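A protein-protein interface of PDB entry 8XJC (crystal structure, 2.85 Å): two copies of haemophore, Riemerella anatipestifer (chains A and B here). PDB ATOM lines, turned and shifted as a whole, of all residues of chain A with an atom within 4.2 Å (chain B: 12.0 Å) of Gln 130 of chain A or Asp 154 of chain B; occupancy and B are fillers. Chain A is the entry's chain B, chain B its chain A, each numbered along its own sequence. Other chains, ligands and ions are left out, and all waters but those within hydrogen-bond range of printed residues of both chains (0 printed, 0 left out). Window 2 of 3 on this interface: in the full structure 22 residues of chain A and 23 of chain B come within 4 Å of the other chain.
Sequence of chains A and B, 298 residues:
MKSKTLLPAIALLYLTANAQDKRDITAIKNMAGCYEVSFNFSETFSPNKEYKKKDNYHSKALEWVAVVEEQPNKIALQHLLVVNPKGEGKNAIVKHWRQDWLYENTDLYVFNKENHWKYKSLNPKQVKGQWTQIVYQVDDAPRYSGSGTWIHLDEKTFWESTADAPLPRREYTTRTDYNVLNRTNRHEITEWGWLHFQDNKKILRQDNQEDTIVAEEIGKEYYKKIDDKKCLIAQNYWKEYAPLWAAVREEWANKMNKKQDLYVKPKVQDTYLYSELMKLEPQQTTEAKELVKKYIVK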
ATOM      1  N   TYR A 103     -35.449  12.248 -15.354  1.00  0.00           N
ATOM      2  CA  TYR A 103     -35.012  10.930 -14.946  1.00  0.00           C
ATOM      3  C   TYR A 103     -36.098   9.929 -14.811  1.00  0.00           C
ATOM      4  O   TYR A 103     -37.095  10.184 -14.163  1.00  0.00           O
ATOM      5  CB  TYR A 103     -34.252  11.049 -13.635  1.00  0.00           C
ATOM      6  CG  TYR A 103     -33.556   9.826 -13.096  1.00  0.00           C
ATOM      7  CD1 TYR A 103     -32.516   9.233 -13.780  1.00  0.00           C
ATOM      8  CD2 TYR A 103     -33.900   9.309 -11.864  1.00  0.00           C
ATOM      9  CE1 TYR A 103     -31.867   8.132 -13.271  1.00  0.00           C
ATOM     10  CE2 TYR A 103     -33.256   8.211 -11.348  1.00  0.00           C
ATOM     11  CZ  TYR A 103     -32.242   7.626 -12.057  1.00  0.00           C
ATOM     12  OH  TYR A 103     -31.607   6.532 -11.540  1.00  0.00           O
ATOM     13  N   GLU A 104     -35.901   8.774 -15.418  1.00  0.00           N
ATOM     14  CA  GLU A 104     -36.878   7.722 -15.387  1.00  0.00           C
ATOM     15  C   GLU A 104     -38.236   8.199 -15.811  1.00  0.00           C
ATOM     16  O   GLU A 104     -39.222   7.969 -15.140  1.00  0.00           O
ATOM     17  CB  GLU A 104     -36.817   6.991 -14.067  1.00  0.00           C
ATOM     18  CG  GLU A 104     -35.488   6.298 -13.854  1.00  0.00           C
ATOM     19  CD  GLU A 104     -35.389   5.607 -12.516  1.00  0.00           C
ATOM     20  OE1 GLU A 104     -36.147   5.967 -11.601  1.00  0.00           O
ATOM     21  OE2 GLU A 104     -34.540   4.712 -12.373  1.00  0.00           O
ATOM     22  N   GLN A 126     -37.774  -0.244 -18.760  1.00  0.00           N
ATOM     23  CA  GLN A 126     -36.634  -0.036 -19.617  1.00  0.00           C
ATOM     24  C   GLN A 126     -35.996   1.302 -19.347  1.00  0.00           C
ATOM     25  O   GLN A 126     -34.844   1.504 -19.682  1.00  0.00           O
ATOM     26  CB  GLN A 126     -37.052  -0.170 -21.067  1.00  0.00           C
ATOM     27  CG  GLN A 126     -37.571  -1.558 -21.427  1.00  0.00           C
ATOM     28  CD  GLN A 126     -36.570  -2.673 -21.152  1.00  0.00           C
ATOM     29  OE1 GLN A 126     -35.384  -2.554 -21.452  1.00  0.00           O
ATOM     30  NE2 GLN A 126     -37.055  -3.777 -20.595  1.00  0.00           N
ATOM     31  N   VAL A 127     -36.726   2.203 -18.704  1.00  0.00           N
ATOM     32  CA  VAL A 127     -36.235   3.541 -18.459  1.00  0.00           C
ATOM     33  C   VAL A 127     -35.576   3.686 -17.124  1.00  0.00           C
ATOM     34  O   VAL A 127     -35.210   4.770 -16.737  1.00  0.00           O
ATOM     35  CB  VAL A 127     -37.350   4.560 -18.604  1.00  0.00           C
ATOM     36  CG1 VAL A 127     -37.889   4.544 -20.015  1.00  0.00           C
ATOM     37  CG2 VAL A 127     -38.454   4.289 -17.606  1.00  0.00           C
ATOM     38  N   LYS A 128     -35.378   2.582 -16.438  1.00  0.00           N
ATOM     39  CA  LYS A 128     -34.699   2.600 -15.169  1.00  0.00           C
ATOM     40  C   LYS A 128     -33.255   2.971 -15.319  1.00  0.00           C
ATOM     41  O   LYS A 128     -32.539   2.345 -16.080  1.00  0.00           O
ATOM     42  CB  LYS A 128     -34.831   1.239 -14.520  1.00  0.00           C
ATOM     43  CG  LYS A 128     -34.050   1.023 -13.244  1.00  0.00           C
ATOM     44  CD  LYS A 128     -34.388  -0.337 -12.672  1.00  0.00           C
ATOM     45  CE  LYS A 128     -33.486  -0.703 -11.513  1.00  0.00           C
ATOM     46  NZ  LYS A 128     -32.130  -1.085 -11.985  1.00  0.00           N
ATOM     47  N   GLY A 129     -32.811   3.988 -14.596  1.00  0.00           N
ATOM     48  CA  GLY A 129     -31.442   4.444 -14.677  1.00  0.00           C
ATOM     49  C   GLY A 129     -31.244   5.400 -15.795  1.00  0.00           C
ATOM     50  O   GLY A 129     -30.186   5.976 -15.931  1.00  0.00           O
ATOM     51  N   GLN A 130     -32.278   5.604 -16.579  1.00  0.00           N
ATOM     52  CA  GLN A 130     -32.178   6.440 -17.735  1.00  0.00           C
ATOM     53  C   GLN A 130     -32.681   7.826 -17.548  1.00  0.00           C
ATOM     54  O   GLN A 130     -33.468   8.091 -16.669  1.00  0.00           O
ATOM     55  CB  GLN A 130     -32.940   5.794 -18.873  1.00  0.00           C
ATOM     56  CG  GLN A 130     -32.400   4.469 -19.357  1.00  0.00           C
ATOM     57  CD  GLN A 130     -33.042   4.056 -20.653  1.00  0.00           C
ATOM     58  OE1 GLN A 130     -34.007   4.662 -21.092  1.00  0.00           O
ATOM     59  NE2 GLN A 130     -32.513   3.020 -21.270  1.00  0.00           N
ATOM     60  N   TRP A 131     -32.211   8.728 -18.383  1.00  0.00           N
ATOM     61  CA  TRP A 131     -32.658  10.088 -18.343  1.00  0.00           C
ATOM     62  C   TRP A 131     -33.213  10.362 -19.705  1.00  0.00           C
ATOM     63  O   TRP A 131     -32.640   9.972 -20.691  1.00  0.00           O
ATOM     64  CB  TRP A 131     -31.500  11.044 -18.112  1.00  0.00           C
ATOM     65  CG  TRP A 131     -30.969  11.191 -16.747  1.00  0.00           C
ATOM     66  CD1 TRP A 131     -30.048  10.408 -16.148  1.00  0.00           C
ATOM     67  CD2 TRP A 131     -31.263  12.241 -15.826  1.00  0.00           C
ATOM     68  NE1 TRP A 131     -29.767  10.878 -14.897  1.00  0.00           N
ATOM     69  CE2 TRP A 131     -30.503  12.008 -14.675  1.00  0.00           C
ATOM     70  CE3 TRP A 131     -32.109  13.348 -15.858  1.00  0.00           C
ATOM     71  CZ2 TRP A 131     -30.565  12.832 -13.565  1.00  0.00           C
ATOM     72  CZ3 TRP A 131     -32.168  14.164 -14.759  1.00  0.00           C
ATOM     73  CH2 TRP A 131     -31.403  13.905 -13.629  1.00  0.00           C
ATOM     74  N   SER A 147     -34.404   8.760 -24.636  1.00  0.00           N
ATOM     75  CA  SER A 147     -33.954   8.324 -23.300  1.00  0.00           C
ATOM     76  C   SER A 147     -32.715   7.457 -23.304  1.00  0.00           C
ATOM     77  O   SER A 147     -32.531   6.648 -24.188  1.00  0.00           O
ATOM     78  CB  SER A 147     -35.052   7.604 -22.540  1.00  0.00           C
ATOM     79  OG  SER A 147     -34.742   7.487 -21.170  1.00  0.00           O
ATOM     80  N   GLY A 148     -31.882   7.609 -22.292  1.00  0.00           N
ATOM     81  CA  GLY A 148     -30.666   6.845 -22.191  1.00  0.00           C
ATOM     82  C   GLY A 148     -29.949   6.969 -20.892  1.00  0.00           C
ATOM     83  O   GLY A 148     -30.241   7.839 -20.114  1.00  0.00           O
ATOM     84  N   THR A 149     -28.998   6.094 -20.654  1.00  0.00           N
ATOM     85  CA  THR A 149     -28.246   6.105 -19.428  1.00  0.00           C
ATOM     86  C   THR A 149     -26.922   6.810 -19.593  1.00  0.00           C
ATOM     87  O   THR A 149     -26.263   6.634 -20.599  1.00  0.00           O
ATOM     88  CB  THR A 149     -28.024   4.667 -18.916  1.00  0.00           C
ATOM     89  OG1 THR A 149     -29.273   3.993 -18.782  1.00  0.00           O
ATOM     90  CG2 THR A 149     -27.321   4.653 -17.584  1.00  0.00           C
ATOM     91  N   ASP B  21     -18.889  -9.665 -16.079  1.00  0.00           N
ATOM     92  CA  ASP B  21     -20.294  -9.430 -15.946  1.00  0.00           C
ATOM     93  C   ASP B  21     -20.877 -10.655 -16.510  1.00  0.00           C
ATOM     94  O   ASP B  21     -22.096 -10.771 -16.515  1.00  0.00           O
ATOM     95  CB  ASP B  21     -20.751  -8.253 -16.789  1.00  0.00           C
ATOM     96  CG  ASP B  21     -22.070  -7.683 -16.357  1.00  0.00           C
ATOM     97  OD1 ASP B  21     -22.709  -8.235 -15.446  1.00  0.00           O
ATOM     98  OD2 ASP B  21     -22.472  -6.662 -16.936  1.00  0.00           O
ATOM     99  N   ARG B  23     -21.842 -11.390 -19.024  1.00  0.00           N
ATOM    100  CA  ARG B  23     -22.407 -10.931 -20.260  1.00  0.00           C
ATOM    101  C   ARG B  23     -21.275 -10.407 -21.085  1.00  0.00           C
ATOM    102  O   ARG B  23     -21.397 -10.271 -22.286  1.00  0.00           O
ATOM    103  CB  ARG B  23     -23.434  -9.857 -19.967  1.00  0.00           C
ATOM    104  CG  ARG B  23     -24.615 -10.317 -19.150  1.00  0.00           C
ATOM    105  CD  ARG B  23     -25.619  -9.195 -19.004  1.00  0.00           C
ATOM    106  NE  ARG B  23     -25.116  -8.131 -18.151  1.00  0.00           N
ATOM    107  CZ  ARG B  23     -25.764  -6.999 -17.923  1.00  0.00           C
ATOM    108  NH1 ARG B  23     -26.932  -6.785 -18.499  1.00  0.00           N
ATOM    109  NH2 ARG B  23     -25.240  -6.080 -17.135  1.00  0.00           N
ATOM    110  N   TRP B 150     -16.992  -3.196 -21.490  1.00  0.00           N
ATOM    111  CA  TRP B 150     -18.150  -3.559 -22.262  1.00  0.00           C
ATOM    112  C   TRP B 150     -19.377  -3.005 -21.594  1.00  0.00           C
ATOM    113  O   TRP B 150     -19.574  -3.199 -20.427  1.00  0.00           O
ATOM    114  CB  TRP B 150     -18.269  -5.067 -22.352  1.00  0.00           C
ATOM    115  CG  TRP B 150     -17.541  -5.718 -23.446  1.00  0.00           C
ATOM    116  CD1 TRP B 150     -16.314  -6.282 -23.382  1.00  0.00           C
ATOM    117  CD2 TRP B 150     -18.009  -5.916 -24.779  1.00  0.00           C
ATOM    118  NE1 TRP B 150     -15.973  -6.804 -24.596  1.00  0.00           N
ATOM    119  CE2 TRP B 150     -17.001  -6.590 -25.474  1.00  0.00           C
ATOM    120  CE3 TRP B 150     -19.178  -5.576 -25.455  1.00  0.00           C
ATOM    121  CZ2 TRP B 150     -17.122  -6.931 -26.808  1.00  0.00           C
ATOM    122  CZ3 TRP B 150     -19.296  -5.913 -26.777  1.00  0.00           C
ATOM    123  CH2 TRP B 150     -18.277  -6.583 -27.442  1.00  0.00           C
ATOM    124  N   ILE B 151     -20.209  -2.303 -22.341  1.00  0.00           N
ATOM    125  CA  ILE B 151     -21.411  -1.702 -21.802  1.00  0.00           C
ATOM    126  C   ILE B 151     -22.615  -2.542 -22.125  1.00  0.00           C
ATOM    127  O   ILE B 151     -22.792  -2.952 -23.253  1.00  0.00           O
ATOM    128  CB  ILE B 151     -21.613  -0.274 -22.335  1.00  0.00           C
ATOM    129  CG1 ILE B 151     -20.353   0.559 -22.142  1.00  0.00           C
ATOM    130  CG2 ILE B 151     -22.792   0.393 -21.659  1.00  0.00           C
ATOM    131  CD1 ILE B 151     -20.022   0.820 -20.696  1.00  0.00           C
ATOM    132  N   HIS B 152     -23.444  -2.804 -21.127  1.00  0.00           N
ATOM    133  CA  HIS B 152     -24.596  -3.632 -21.315  1.00  0.00           C
ATOM    134  C   HIS B 152     -25.729  -2.866 -20.757  1.00  0.00           C
ATOM    135  O   HIS B 152     -26.285  -3.230 -19.746  1.00  0.00           O
ATOM    136  CB  HIS B 152     -24.430  -4.889 -20.507  1.00  0.00           C
ATOM    137  CG  HIS B 152     -23.233  -5.696 -20.871  1.00  0.00           C
ATOM    138  ND1 HIS B 152     -23.199  -6.512 -21.977  1.00  0.00           N
ATOM    139  CD2 HIS B 152     -22.033  -5.824 -20.268  1.00  0.00           C
ATOM    140  CE1 HIS B 152     -22.019  -7.094 -22.049  1.00  0.00           C
ATOM    141  NE2 HIS B 152     -21.294  -6.696 -21.023  1.00  0.00           N
ATOM    142  N   LEU B 153     -26.100  -1.798 -21.426  1.00  0.00           N
ATOM    143  CA  LEU B 153     -27.135  -0.937 -20.933  1.00  0.00           C
ATOM    144  C   LEU B 153     -27.966  -0.440 -22.076  1.00  0.00           C
ATOM    145  O   LEU B 153     -27.522  -0.477 -23.200  1.00  0.00           O
ATOM    146  CB  LEU B 153     -26.535   0.254 -20.192  1.00  0.00           C
ATOM    147  CG  LEU B 153     -25.923   0.112 -18.807  1.00  0.00           C
ATOM    148  CD1 LEU B 153     -25.142   1.368 -18.482  1.00  0.00           C
ATOM    149  CD2 LEU B 153     -27.015  -0.109 -17.782  1.00  0.00           C
ATOM    150  N   ASP B 154     -29.177   0.007 -21.796  1.00  0.00           N
ATOM    151  CA  ASP B 154     -30.070   0.565 -22.802  1.00  0.00           C
ATOM    152  C   ASP B 154     -30.387  -0.409 -23.905  1.00  0.00           C
ATOM    153  O   ASP B 154     -30.687   0.005 -25.009  1.00  0.00           O
ATOM    154  CB  ASP B 154     -29.544   1.893 -23.330  1.00  0.00           C
ATOM    155  CG  ASP B 154     -29.268   2.881 -22.249  1.00  0.00           C
ATOM    156  OD1 ASP B 154     -29.718   2.663 -21.116  1.00  0.00           O
ATOM    157  OD2 ASP B 154     -28.598   3.884 -22.540  1.00  0.00           O
ATOM    158  N   GLU B 155     -30.376  -1.693 -23.587  1.00  0.00           N
ATOM    159  CA  GLU B 155     -30.636  -2.743 -24.572  1.00  0.00           C
ATOM    160  C   GLU B 155     -29.588  -2.752 -25.637  1.00  0.00           C
ATOM    161  O   GLU B 155     -29.816  -3.207 -26.744  1.00  0.00           O
ATOM    162  CB  GLU B 155     -32.048  -2.709 -25.120  1.00  0.00           C
ATOM    163  CG  GLU B 155     -33.077  -3.299 -24.175  1.00  0.00           C
ATOM    164  CD  GLU B 155     -34.415  -3.524 -24.844  1.00  0.00           C
ATOM    165  OE1 GLU B 155     -34.706  -2.825 -25.836  1.00  0.00           O
ATOM    166  OE2 GLU B 155     -35.177  -4.401 -24.380  1.00  0.00           O
ATOM    167  N   LYS B 156     -28.414  -2.268 -25.285  1.00  0.00           N
ATOM    168  CA  LYS B 156     -27.337  -2.213 -26.222  1.00  0.00           C
ATOM    169  C   LYS B 156     -26.124  -2.879 -25.628  1.00  0.00           C
ATOM    170  O   LYS B 156     -25.877  -2.755 -24.449  1.00  0.00           O
ATOM    171  CB  LYS B 156     -27.050  -0.762 -26.565  1.00  0.00           C
ATOM    172  CG  LYS B 156     -28.133  -0.062 -27.360  1.00  0.00           C
ATOM    173  CD  LYS B 156     -27.977   1.444 -27.269  1.00  0.00           C
ATOM    174  CE  LYS B 156     -26.582   1.878 -27.675  1.00  0.00           C
ATOM    175  NZ  LYS B 156     -26.348   3.323 -27.414  1.00  0.00           N
ATOM    176  N   THR B 157     -25.374  -3.602 -26.442  1.00  0.00           N
ATOM    177  CA  THR B 157     -24.166  -4.256 -25.989  1.00  0.00           C
ATOM    178  C   THR B 157     -22.995  -3.739 -26.785  1.00  0.00           C
ATOM    179  O   THR B 157     -22.807  -4.115 -27.919  1.00  0.00           O
ATOM    180  CB  THR B 157     -24.271  -5.770 -26.114  1.00  0.00           C
ATOM    181  OG1 THR B 157     -25.447  -6.222 -25.436  1.00  0.00           O
ATOM    182  CG2 THR B 157     -23.069  -6.433 -25.500  1.00  0.00           C
ATOM    183  N   PHE B 158     -22.192  -2.880 -26.175  1.00  0.00           N
ATOM    184  CA  PHE B 158     -21.079  -2.293 -26.878  1.00  0.00           C
ATOM    185  C   PHE B 158     -19.750  -2.121 -26.172  1.00  0.00           C
ATOM    186  O   PHE B 158     -19.699  -2.106 -24.971  1.00  0.00           O
ATOM    187  CB  PHE B 158     -21.507  -0.993 -27.566  1.00  0.00           C
ATOM    188  CG  PHE B 158     -21.801   0.144 -26.652  1.00  0.00           C
ATOM    189  CD1 PHE B 158     -23.071   0.334 -26.159  1.00  0.00           C
ATOM    190  CD2 PHE B 158     -20.823   1.065 -26.349  1.00  0.00           C
ATOM    191  CE1 PHE B 158     -23.352   1.397 -25.339  1.00  0.00           C
ATOM    192  CE2 PHE B 158     -21.093   2.129 -25.529  1.00  0.00           C
ATOM    193  CZ  PHE B 158     -22.362   2.298 -25.024  1.00  0.00           C
ATOM    194  N   TRP B 159     -18.674  -1.991 -26.938  1.00  0.00           N
ATOM    195  CA  TRP B 159     -17.346  -1.771 -26.402  1.00  0.00           C
ATOM    196  C   TRP B 159     -16.665  -0.742 -27.260  1.00  0.00           C
ATOM    197  O   TRP B 159     -16.708  -0.844 -28.462  1.00  0.00           O
ATOM    198  CB  TRP B 159     -16.546  -3.042 -26.528  1.00  0.00           C
ATOM    199  CG  TRP B 159     -15.142  -3.004 -26.042  1.00  0.00           C
ATOM    200  CD1 TRP B 159     -14.717  -3.206 -24.775  1.00  0.00           C
ATOM    201  CD2 TRP B 159     -13.968  -2.798 -26.832  1.00  0.00           C
ATOM    202  NE1 TRP B 159     -13.355  -3.124 -24.714  1.00  0.00           N
ATOM    203  CE2 TRP B 159     -12.870  -2.867 -25.966  1.00  0.00           C
ATOM    204  CE3 TRP B 159     -13.739  -2.550 -28.188  1.00  0.00           C
ATOM    205  CZ2 TRP B 159     -11.567  -2.705 -26.404  1.00  0.00           C
ATOM    206  CZ3 TRP B 159     -12.451  -2.383 -28.617  1.00  0.00           C
ATOM    207  CH2 TRP B 159     -11.379  -2.465 -27.732  1.00  0.00           C
ATOM    208  N   GLU B 160     -15.993   0.223 -26.655  1.00  0.00           N
ATOM    209  CA  GLU B 160     -15.278   1.236 -27.400  1.00  0.00           C
ATOM    210  C   GLU B 160     -13.890   1.522 -26.869  1.00  0.00           C
ATOM    211  O   GLU B 160     -13.673   1.500 -25.677  1.00  0.00           O
ATOM    212  CB  GLU B 160     -16.116   2.505 -27.393  1.00  0.00           C
ATOM    213  CG  GLU B 160     -15.903   3.479 -28.527  1.00  0.00           C
ATOM    214  CD  GLU B 160     -16.967   4.546 -28.511  1.00  0.00           C
ATOM    215  OE1 GLU B 160     -17.821   4.494 -27.605  1.00  0.00           O
ATOM    216  OE2 GLU B 160     -16.959   5.428 -29.396  1.00  0.00           O
ATOM    217  N   ARG B 186     -15.629   0.880 -32.217  1.00  0.00           N
ATOM    218  CA  ARG B 186     -16.808   0.475 -31.477  1.00  0.00           C
ATOM    219  C   ARG B 186     -17.307  -0.835 -31.963  1.00  0.00           C
ATOM    220  O   ARG B 186     -17.590  -0.999 -33.124  1.00  0.00           O
ATOM    221  CB  ARG B 186     -17.924   1.486 -31.612  1.00  0.00           C
ATOM    222  CG  ARG B 186     -19.153   1.220 -30.772  1.00  0.00           C
ATOM    223  CD  ARG B 186     -20.224   2.215 -31.163  1.00  0.00           C
ATOM    224  NE  ARG B 186     -21.522   1.942 -30.566  1.00  0.00           N
ATOM    225  CZ  ARG B 186     -22.026   2.616 -29.545  1.00  0.00           C
ATOM    226  NH1 ARG B 186     -21.344   3.603 -28.997  1.00  0.00           N
ATOM    227  NH2 ARG B 186     -23.219   2.304 -29.079  1.00  0.00           N
ATOM    228  N   GLU B 188     -20.273  -3.360 -31.562  1.00  0.00           N
ATOM    229  CA  GLU B 188     -21.603  -3.484 -31.043  1.00  0.00           C
ATOM    230  C   GLU B 188     -22.309  -4.715 -31.515  1.00  0.00           C
ATOM    231  O   GLU B 188     -22.309  -5.010 -32.688  1.00  0.00           O
ATOM    232  CB  GLU B 188     -22.439  -2.265 -31.394  1.00  0.00           C
ATOM    233  CG  GLU B 188     -23.814  -2.270 -30.761  1.00  0.00           C
ATOM    234  CD  GLU B 188     -24.503  -0.934 -30.843  1.00  0.00           C
ATOM    235  OE1 GLU B 188     -23.816   0.079 -31.058  1.00  0.00           O
ATOM    236  OE2 GLU B 188     -25.736  -0.900 -30.680  1.00  0.00           O
ATOM    237  N   ILE B 189     -22.925  -5.435 -30.596  1.00  0.00           N
ATOM    238  CA  ILE B 189     -23.681  -6.611 -30.952  1.00  0.00           C
ATOM    239  C   ILE B 189     -25.068  -6.221 -31.368  1.00  0.00           C
ATOM    240  O   ILE B 189     -25.714  -5.430 -30.705  1.00  0.00           O
ATOM    241  CB  ILE B 189     -23.679  -7.667 -29.836  1.00  0.00           C
ATOM    242  CG1 ILE B 189     -22.260  -7.926 -29.351  1.00  0.00           C
ATOM    243  CG2 ILE B 189     -24.301  -8.965 -30.310  1.00  0.00           C
ATOM    244  CD1 ILE B 189     -21.374  -8.550 -30.398  1.00  0.00           C
ATOM    245  N   THR B 190     -25.530  -6.782 -32.471  1.00  0.00           N
ATOM    246  CA  THR B 190     -26.822  -6.456 -33.034  1.00  0.00           C
ATOM    247  C   THR B 190     -27.592  -7.741 -33.277  1.00  0.00           C
ATOM    248  O   THR B 190     -27.045  -8.818 -33.163  1.00  0.00           O
ATOM    249  CB  THR B 190     -26.650  -5.727 -34.367  1.00  0.00           C
ATOM    250  OG1 THR B 190     -26.075  -6.607 -35.322  1.00  0.00           O
ATOM    251  CG2 THR B 190     -25.757  -4.517 -34.216  1.00  0.00           C
ATOM    252  N   GLU B 191     -28.878  -7.640 -33.537  1.00  0.00           N
ATOM    253  CA  GLU B 191     -29.691  -8.815 -33.813  1.00  0.00           C
ATOM    254  C   GLU B 191     -29.257  -9.539 -35.053  1.00  0.00           C
ATOM    255  O   GLU B 191     -29.291 -10.754 -35.101  1.00  0.00           O
ATOM    256  CB  GLU B 191     -31.146  -8.427 -33.941  1.00  0.00           C
ATOM    257  CG  GLU B 191     -31.868  -8.337 -32.607  1.00  0.00           C
ATOM    258  CD  GLU B 191     -33.345  -8.660 -32.719  1.00  0.00           C
ATOM    259  OE1 GLU B 191     -33.812  -8.933 -33.845  1.00  0.00           O
ATOM    260  OE2 GLU B 191     -34.039  -8.647 -31.681  1.00  0.00           O
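NE2 of Gln 130 of chain A lies within hydrogen-bond range of OD1 of Asp 154 of chain B (2.8 Å). The side-chain hydroxyl of Thr 149 of chain A is in hydrogen-bond range of the side-chain carboxylate of Asp 154 of chain B (2.7 Å). The side-chain amide oxygen of Gln 126 of chain A lies close to the side-chain carboxylate of Glu 155 of chain B, at 3.5 Å.
Along chain A the printed residues that touch a printed residue of chain B span positions 126 to 149. Among the printed residues, 4 pairs touch across the chains. Among the printed residues, no Asp or Glu carboxylate lies within 4 Å of a Lys or Arg side-chain nitrogen of the other chain.
No position is printed for both chains.
The backbone carbonyl oxygen of Gln 130 of chain A is in hydrogen-bond range of the backbone NH of Glu 104 of chain A (2.8 Å). NE2 of Gln 130 of chain A is in hydrogen-bond range of O of Gln 126 of chain A (3.2 Å). OE1 of Gln 130 of chain A is in hydrogen-bond range of OG of Ser 147 of chain A (2.9 Å). The backbone NH (N) of Trp 131 of chain A sits at hydrogen-bond distance from the backbone carbonyl oxygen (O) of Gly 148 of chain A (2.8 Å).
Among the printed residues, pairs that only touch across the chains: Gly 148 of chain A with Asp 154 of chain B.
Gln 130 of chain A touches one residue of chain B. Of chain A, only Gln 130, Gly 148 and Thr 149 come within 4 Å of Asp 154 of chain B. No residue of chain B comes within 4 Å of Tyr 103 of chain A. No residue of chain B comes within 4 Å of Val 127 of chain A. Gly 129 of chain A touches none of the printed residues of chain B. No residue of chain B comes within 4 Å of Trp 131 of chain A. No residue of chain B comes within 4 Å of Ser 147 of chain A. Gly 148 of chain A touches just one residue of chain B: Asp 154 (3.6 Å). Thr 149 of chain A touches just one residue of chain B: Asp 154 (2.7 Å). Of the printed residues of chain A, Glu 155 of chain B touches Gln 126. Of the printed residues of chain B, Gln 126 of chain A touches Glu 155. Glu 191 of chain B touches none of the printed residues of chain A. Lys 128 of chain A touches none of the printed residues of chain B. The nearest printed residue of chain A that does not touch Asp 154 of chain B is Ser 147 of chain A (5.1 Å). The nearest printed residue of chain A that does not touch Glu 155 of chain B is Gln 130 of chain A (5.7 Å).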
